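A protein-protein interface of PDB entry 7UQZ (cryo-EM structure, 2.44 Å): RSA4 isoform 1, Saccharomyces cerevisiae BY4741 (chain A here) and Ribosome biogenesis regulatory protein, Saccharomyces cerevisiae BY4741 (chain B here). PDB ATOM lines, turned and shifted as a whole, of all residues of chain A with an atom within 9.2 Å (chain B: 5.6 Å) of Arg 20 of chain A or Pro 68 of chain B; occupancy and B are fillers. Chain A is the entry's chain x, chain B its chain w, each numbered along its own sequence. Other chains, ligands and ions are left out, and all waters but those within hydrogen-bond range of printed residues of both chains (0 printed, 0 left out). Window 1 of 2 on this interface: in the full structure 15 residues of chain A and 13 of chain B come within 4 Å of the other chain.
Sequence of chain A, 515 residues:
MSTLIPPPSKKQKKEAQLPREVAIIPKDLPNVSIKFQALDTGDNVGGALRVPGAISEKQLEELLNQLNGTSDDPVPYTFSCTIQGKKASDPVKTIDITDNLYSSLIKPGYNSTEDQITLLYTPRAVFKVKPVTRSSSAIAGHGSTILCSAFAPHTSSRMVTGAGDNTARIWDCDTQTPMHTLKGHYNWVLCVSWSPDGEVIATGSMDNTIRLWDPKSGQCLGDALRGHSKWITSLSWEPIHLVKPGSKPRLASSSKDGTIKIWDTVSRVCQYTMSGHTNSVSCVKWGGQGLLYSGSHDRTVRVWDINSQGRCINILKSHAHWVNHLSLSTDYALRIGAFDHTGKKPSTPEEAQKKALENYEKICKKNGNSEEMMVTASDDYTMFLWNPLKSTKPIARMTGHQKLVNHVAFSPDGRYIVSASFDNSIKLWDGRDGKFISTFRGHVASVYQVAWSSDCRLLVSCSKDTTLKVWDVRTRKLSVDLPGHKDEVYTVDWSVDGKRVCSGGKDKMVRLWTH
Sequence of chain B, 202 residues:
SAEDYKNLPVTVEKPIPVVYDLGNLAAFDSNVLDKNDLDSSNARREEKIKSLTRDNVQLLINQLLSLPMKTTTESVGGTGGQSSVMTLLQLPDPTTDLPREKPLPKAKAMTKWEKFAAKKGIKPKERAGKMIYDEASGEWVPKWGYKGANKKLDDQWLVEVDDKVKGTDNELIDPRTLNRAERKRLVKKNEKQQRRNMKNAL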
ATOM      1  N   GLN A  12      13.484 -16.132   7.521  1.00  0.00           N
ATOM      2  CA  GLN A  12      14.714 -16.839   7.179  1.00  0.00           C
ATOM      3  C   GLN A  12      15.265 -16.380   5.834  1.00  0.00           C
ATOM      4  O   GLN A  12      16.483 -16.291   5.655  1.00  0.00           O
ATOM      5  CB  GLN A  12      14.466 -18.347   7.186  1.00  0.00           C
ATOM      6  CG  GLN A  12      14.232 -18.916   8.579  1.00  0.00           C
ATOM      7  CD  GLN A  12      13.711 -20.336   8.552  1.00  0.00           C
ATOM      8  OE1 GLN A  12      13.096 -20.766   7.577  1.00  0.00           O
ATOM      9  NE2 GLN A  12      13.952 -21.076   9.627  1.00  0.00           N
ATOM     10  N   LYS A  14      14.854 -13.333   4.644  1.00  0.00           N
ATOM     11  CA  LYS A  14      15.446 -12.034   4.957  1.00  0.00           C
ATOM     12  C   LYS A  14      16.817 -12.187   5.613  1.00  0.00           C
ATOM     13  O   LYS A  14      17.752 -11.437   5.306  1.00  0.00           O
ATOM     14  CB  LYS A  14      14.509 -11.233   5.860  1.00  0.00           C
ATOM     15  CG  LYS A  14      13.267 -10.707   5.164  1.00  0.00           C
ATOM     16  CD  LYS A  14      13.619  -9.633   4.146  1.00  0.00           C
ATOM     17  CE  LYS A  14      14.410  -8.498   4.785  1.00  0.00           C
ATOM     18  NZ  LYS A  14      13.682  -7.889   5.933  1.00  0.00           N
ATOM     19  N   GLU A  15      16.951 -13.153   6.525  1.00  0.00           N
ATOM     20  CA  GLU A  15      18.245 -13.405   7.153  1.00  0.00           C
ATOM     21  C   GLU A  15      19.269 -13.887   6.132  1.00  0.00           C
ATOM     22  O   GLU A  15      20.457 -13.558   6.230  1.00  0.00           O
ATOM     23  CB  GLU A  15      18.098 -14.427   8.280  1.00  0.00           C
ATOM     24  CG  GLU A  15      17.359 -13.911   9.501  1.00  0.00           C
ATOM     25  CD  GLU A  15      17.269 -14.947  10.605  1.00  0.00           C
ATOM     26  OE1 GLU A  15      18.163 -15.817  10.678  1.00  0.00           O
ATOM     27  OE2 GLU A  15      16.304 -14.895  11.395  1.00  0.00           O
ATOM     28  N   ALA A  16      18.828 -14.686   5.158  1.00  0.00           N
ATOM     29  CA  ALA A  16      19.716 -15.103   4.077  1.00  0.00           C
ATOM     30  C   ALA A  16      20.150 -13.912   3.230  1.00  0.00           C
ATOM     31  O   ALA A  16      21.317 -13.820   2.834  1.00  0.00           O
ATOM     32  CB  ALA A  16      19.027 -16.158   3.212  1.00  0.00           C
ATOM     33  N   GLN A  17      19.225 -12.993   2.944  1.00  0.00           N
ATOM     34  CA  GLN A  17      19.568 -11.805   2.169  1.00  0.00           C
ATOM     35  C   GLN A  17      20.448 -10.835   2.946  1.00  0.00           C
ATOM     36  O   GLN A  17      21.105  -9.987   2.331  1.00  0.00           O
ATOM     37  CB  GLN A  17      18.299 -11.094   1.696  1.00  0.00           C
ATOM     38  CG  GLN A  17      17.575 -11.813   0.573  1.00  0.00           C
ATOM     39  CD  GLN A  17      16.385 -11.036   0.051  1.00  0.00           C
ATOM     40  OE1 GLN A  17      15.788 -11.401  -0.960  1.00  0.00           O
ATOM     41  NE2 GLN A  17      16.031  -9.959   0.741  1.00  0.00           N
ATOM     42  N   LEU A  18      20.458 -10.926   4.275  1.00  0.00           N
ATOM     43  CA  LEU A  18      21.391 -10.139   5.069  1.00  0.00           C
ATOM     44  C   LEU A  18      22.832 -10.531   4.734  1.00  0.00           C
ATOM     45  O   LEU A  18      23.097 -11.678   4.362  1.00  0.00           O
ATOM     46  CB  LEU A  18      21.133 -10.343   6.562  1.00  0.00           C
ATOM     47  CG  LEU A  18      19.949  -9.610   7.190  1.00  0.00           C
ATOM     48  CD1 LEU A  18      19.826  -9.969   8.660  1.00  0.00           C
ATOM     49  CD2 LEU A  18      20.095  -8.109   7.012  1.00  0.00           C
ATOM     50  N   PRO A  19      23.779  -9.594   4.838  1.00  0.00           N
ATOM     51  CA  PRO A  19      25.176  -9.921   4.520  1.00  0.00           C
ATOM     52  C   PRO A  19      25.755 -10.949   5.481  1.00  0.00           C
ATOM     53  O   PRO A  19      25.384 -11.018   6.655  1.00  0.00           O
ATOM     54  CB  PRO A  19      25.895  -8.573   4.644  1.00  0.00           C
ATOM     55  CG  PRO A  19      25.028  -7.764   5.545  1.00  0.00           C
ATOM     56  CD  PRO A  19      23.624  -8.179   5.217  1.00  0.00           C
ATOM     57  N   ARG A  20      26.681 -11.750   4.965  1.00  0.00           N
ATOM     58  CA  ARG A  20      27.263 -12.855   5.707  1.00  0.00           C
ATOM     59  C   ARG A  20      28.573 -12.441   6.369  1.00  0.00           C
ATOM     60  O   ARG A  20      29.332 -11.622   5.848  1.00  0.00           O
ATOM     61  CB  ARG A  20      27.503 -14.049   4.783  1.00  0.00           C
ATOM     62  CG  ARG A  20      26.243 -14.598   4.138  1.00  0.00           C
ATOM     63  CD  ARG A  20      25.397 -15.348   5.147  1.00  0.00           C
ATOM     64  NE  ARG A  20      26.021 -16.603   5.544  1.00  0.00           N
ATOM     65  CZ  ARG A  20      25.574 -17.388   6.512  1.00  0.00           C
ATOM     66  NH1 ARG A  20      24.504 -17.069   7.223  1.00  0.00           N
ATOM     67  NH2 ARG A  20      26.213 -18.524   6.774  1.00  0.00           N
ATOM     68  N   GLU A  21      28.828 -13.025   7.534  1.00  0.00           N
ATOM     69  CA  GLU A  21      30.096 -12.845   8.222  1.00  0.00           C
ATOM     70  C   GLU A  21      31.170 -13.687   7.548  1.00  0.00           C
ATOM     71  O   GLU A  21      30.886 -14.729   6.953  1.00  0.00           O
ATOM     72  CB  GLU A  21      29.974 -13.224   9.702  1.00  0.00           C
ATOM     73  CG  GLU A  21      29.445 -14.631   9.961  1.00  0.00           C
ATOM     74  CD  GLU A  21      30.540 -15.682  10.000  1.00  0.00           C
ATOM     75  OE1 GLU A  21      31.722 -15.307  10.149  1.00  0.00           O
ATOM     76  OE2 GLU A  21      30.218 -16.883   9.879  1.00  0.00           O
ATOM     77  N   VAL A  22      32.412 -13.226   7.646  1.00  0.00           N
ATOM     78  CA  VAL A  22      33.551 -13.900   7.036  1.00  0.00           C
ATOM     79  C   VAL A  22      34.468 -14.382   8.150  1.00  0.00           C
ATOM     80  O   VAL A  22      34.878 -13.596   9.014  1.00  0.00           O
ATOM     81  CB  VAL A  22      34.297 -12.980   6.058  1.00  0.00           C
ATOM     82  CG1 VAL A  22      35.491 -13.703   5.465  1.00  0.00           C
ATOM     83  CG2 VAL A  22      33.358 -12.512   4.958  1.00  0.00           C
ATOM     84  N   ALA A  23      34.779 -15.675   8.138  1.00  0.00           N
ATOM     85  CA  ALA A  23      35.679 -16.272   9.124  1.00  0.00           C
ATOM     86  C   ALA A  23      37.108 -16.077   8.639  1.00  0.00           C
ATOM     87  O   ALA A  23      37.642 -16.870   7.862  1.00  0.00           O
ATOM     88  CB  ALA A  23      35.353 -17.745   9.332  1.00  0.00           C
ATOM     89  N   LEU B  22      23.665 -11.012  -3.658  1.00  0.00           N
ATOM     90  CA  LEU B  22      24.249 -12.308  -3.972  1.00  0.00           C
ATOM     91  C   LEU B  22      23.377 -13.145  -4.898  1.00  0.00           C
ATOM     92  O   LEU B  22      23.881 -14.096  -5.504  1.00  0.00           O
ATOM     93  CB  LEU B  22      24.531 -13.077  -2.680  1.00  0.00           C
ATOM     94  CG  LEU B  22      25.437 -12.342  -1.688  1.00  0.00           C
ATOM     95  CD1 LEU B  22      25.672 -13.177  -0.442  1.00  0.00           C
ATOM     96  CD2 LEU B  22      26.756 -11.969  -2.340  1.00  0.00           C
ATOM     97  N   GLN B  63      32.106 -13.119   0.273  1.00  0.00           N
ATOM     98  CA  GLN B  63      30.711 -13.319   0.662  1.00  0.00           C
ATOM     99  C   GLN B  63      30.153 -14.628   0.107  1.00  0.00           C
ATOM    100  O   GLN B  63      29.465 -15.374   0.819  1.00  0.00           O
ATOM    101  CB  GLN B  63      29.859 -12.139   0.196  1.00  0.00           C
ATOM    102  CG  GLN B  63      30.226 -10.823   0.846  1.00  0.00           C
ATOM    103  CD  GLN B  63      30.026 -10.835   2.349  1.00  0.00           C
ATOM    104  OE1 GLN B  63      29.039 -11.370   2.853  1.00  0.00           O
ATOM    105  NE2 GLN B  63      30.970 -10.248   3.074  1.00  0.00           N
ATOM    106  N   SER B  66      31.416 -17.453   1.985  1.00  0.00           N
ATOM    107  CA  SER B  66      30.814 -17.467   3.310  1.00  0.00           C
ATOM    108  C   SER B  66      29.341 -17.857   3.288  1.00  0.00           C
ATOM    109  O   SER B  66      28.759 -18.067   4.358  1.00  0.00           O
ATOM    110  CB  SER B  66      30.971 -16.096   3.973  1.00  0.00           C
ATOM    111  OG  SER B  66      32.335 -15.719   4.034  1.00  0.00           O
ATOM    112  N   LEU B  67      28.730 -17.949   2.109  1.00  0.00           N
ATOM    113  CA  LEU B  67      27.351 -18.409   2.009  1.00  0.00           C
ATOM    114  C   LEU B  67      27.226 -19.872   2.445  1.00  0.00           C
ATOM    115  O   LEU B  67      28.197 -20.630   2.385  1.00  0.00           O
ATOM    116  CB  LEU B  67      26.843 -18.263   0.576  1.00  0.00           C
ATOM    117  CG  LEU B  67      26.258 -16.919   0.146  1.00  0.00           C
ATOM    118  CD1 LEU B  67      25.722 -17.022  -1.271  1.00  0.00           C
ATOM    119  CD2 LEU B  67      25.162 -16.485   1.102  1.00  0.00           C
ATOM    120  N   PRO B  68      26.043 -20.289   2.899  1.00  0.00           N
ATOM    121  CA  PRO B  68      25.839 -21.703   3.234  1.00  0.00           C
ATOM    122  C   PRO B  68      25.891 -22.593   2.001  1.00  0.00           C
ATOM    123  O   PRO B  68      25.644 -22.168   0.869  1.00  0.00           O
ATOM    124  CB  PRO B  68      24.450 -21.725   3.879  1.00  0.00           C
ATOM    125  CG  PRO B  68      23.782 -20.492   3.391  1.00  0.00           C
ATOM    126  CD  PRO B  68      24.869 -19.474   3.260  1.00  0.00           C
ATOM    127  N   MET B  69      26.230 -23.856   2.243  1.00  0.00           N
ATOM    128  CA  MET B  69      26.512 -24.804   1.176  1.00  0.00           C
ATOM    129  C   MET B  69      25.629 -26.035   1.311  1.00  0.00           C
ATOM    130  O   MET B  69      25.389 -26.528   2.417  1.00  0.00           O
ATOM    131  CB  MET B  69      27.989 -25.207   1.188  1.00  0.00           C
ATOM    132  CG  MET B  69      28.934 -24.024   1.076  1.00  0.00           C
ATOM    133  SD  MET B  69      30.648 -24.414   1.461  1.00  0.00           S
ATOM    134  CE  MET B  69      31.375 -22.780   1.378  1.00  0.00           C
ATOM    135  N   LYS B  70      25.155 -26.522   0.170  1.00  0.00           N
ATOM    136  CA  LYS B  70      24.313 -27.704   0.080  1.00  0.00           C
ATOM    137  C   LYS B  70      25.129 -28.871  -0.457  1.00  0.00           C
ATOM    138  O   LYS B  70      25.839 -28.734  -1.462  1.00  0.00           O
ATOM    139  CB  LYS B  70      23.103 -27.442  -0.820  1.00  0.00           C
ATOM    140  CG  LYS B  70      22.254 -28.670  -1.098  1.00  0.00           C
ATOM    141  CD  LYS B  70      21.028 -28.318  -1.920  1.00  0.00           C
ATOM    142  CE  LYS B  70      20.270 -29.567  -2.337  1.00  0.00           C
ATOM    143  NZ  LYS B  70      19.876 -30.394  -1.164  1.00  0.00           N
ATOM    144  N   LEU B  88      27.397 -27.269  -3.506  1.00  0.00           N
ATOM    145  CA  LEU B  88      26.860 -26.084  -4.156  1.00  0.00           C
ATOM    146  C   LEU B  88      26.660 -24.966  -3.144  1.00  0.00           C
ATOM    147  O   LEU B  88      26.520 -25.211  -1.947  1.00  0.00           O
ATOM    148  CB  LEU B  88      25.530 -26.392  -4.850  1.00  0.00           C
ATOM    149  CG  LEU B  88      25.539 -27.476  -5.929  1.00  0.00           C
ATOM    150  CD1 LEU B  88      24.158 -27.618  -6.544  1.00  0.00           C
ATOM    151  CD2 LEU B  88      26.572 -27.167  -6.995  1.00  0.00           C
ATOM    152  N   LEU B  89      26.664 -23.729  -3.635  1.00  0.00           N
ATOM    153  CA  LEU B  89      26.318 -22.585  -2.804  1.00  0.00           C
ATOM    154  C   LEU B  89      24.811 -22.375  -2.823  1.00  0.00           C
ATOM    155  O   LEU B  89      24.154 -22.617  -3.838  1.00  0.00           O
ATOM    156  CB  LEU B  89      27.025 -21.325  -3.302  1.00  0.00           C
ATOM    157  CG  LEU B  89      28.543 -21.367  -3.471  1.00  0.00           C
ATOM    158  CD1 LEU B  89      29.028 -20.116  -4.187  1.00  0.00           C
ATOM    159  CD2 LEU B  89      29.230 -21.512  -2.127  1.00  0.00           C
ATOM    160  N   GLN B  90      24.255 -21.927  -1.698  1.00  0.00           N
ATOM    161  CA  GLN B  90      22.828 -21.626  -1.608  1.00  0.00           C
ATOM    162  C   GLN B  90      22.649 -20.116  -1.739  1.00  0.00           C
ATOM    163  O   GLN B  90      22.772 -19.376  -0.762  1.00  0.00           O
ATOM    164  CB  GLN B  90      22.239 -22.159  -0.307  1.00  0.00           C
ATOM    165  CG  GLN B  90      22.144 -23.672  -0.265  1.00  0.00           C
ATOM    166  CD  GLN B  90      21.512 -24.181   1.011  1.00  0.00           C
ATOM    167  OE1 GLN B  90      21.893 -23.781   2.109  1.00  0.00           O
ATOM    168  NE2 GLN B  90      20.534 -25.067   0.873  1.00  0.00           N
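Gln 12 of chain A touches none of the printed residues of chain B. Gln 17 of chain A touches none of the printed residues of chain B. Arg 20 of chain A touches four residues of chain B. Of the printed residues of chain B, Glu 21 of chain A touches Ser 66 (3.3 Å). Of the printed residues of chain B, Val 22 of chain A touches Gln 63 (3.8 Å) and Ser 66 (3.5 Å). Printed residues of chain A within 4 Å of Gln 63 of chain B: Arg 20 and Val 22. Printed residues of chain A within 4 Å of Ser 66 of chain B: Arg 20, Glu 21 and Val 22. Printed residues of chain A within 4 Å of Leu 67 of chain B: Arg 20 (3.7 Å).
Hydrophobic or aromatic side chains of chain B within 4 Å of the printed part of chain A: Leu 67 and Pro 68. Of the 11 printed residues of chain A, 3 touch a printed residue of chain B. Printed residues of chain A that touch a printed residue of chain B: Arg 20, Glu 21 and Val 22. Hydrophobic or aromatic side chains of chain A that line the printed part of chain B: Val 22. Among the printed residues, no Asp or Glu carboxylate lies within 4 Å of a Lys or Arg side-chain nitrogen of the other chain.
Arg 20 of chain A touches Leu 67 of chain B (CG to CD2, 3.7 Å). Pro 68 of chain B touches Arg 20 of chain A. Val 22 of chain A touches Gln 63 of chain B (CG2 to NE2, 3.8 Å). CG2 of Val 22 of chain A touches OG of Ser 66 of chain B, at 3.5 Å.
O of Pro 68 of chain B is in hydrogen-bond range of N of Gln 90 of chain B (2.9 Å).
The side-chain amide oxygen of Gln 63 of chain B sits close to the backbone carbonyl oxygen of Arg 20 of chain A (3.0 Å). The backbone carbonyl oxygen of Ser 66 of chain B sits at hydrogen-bond distance from the guanidinium group of Arg 20 of chain A (3.3 Å). The side-chain hydroxyl (OG) of Ser 66 of chain B sits close to the backbone carbonyl oxygen (O) of Glu 21 of chain A, 3.4 Å away.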
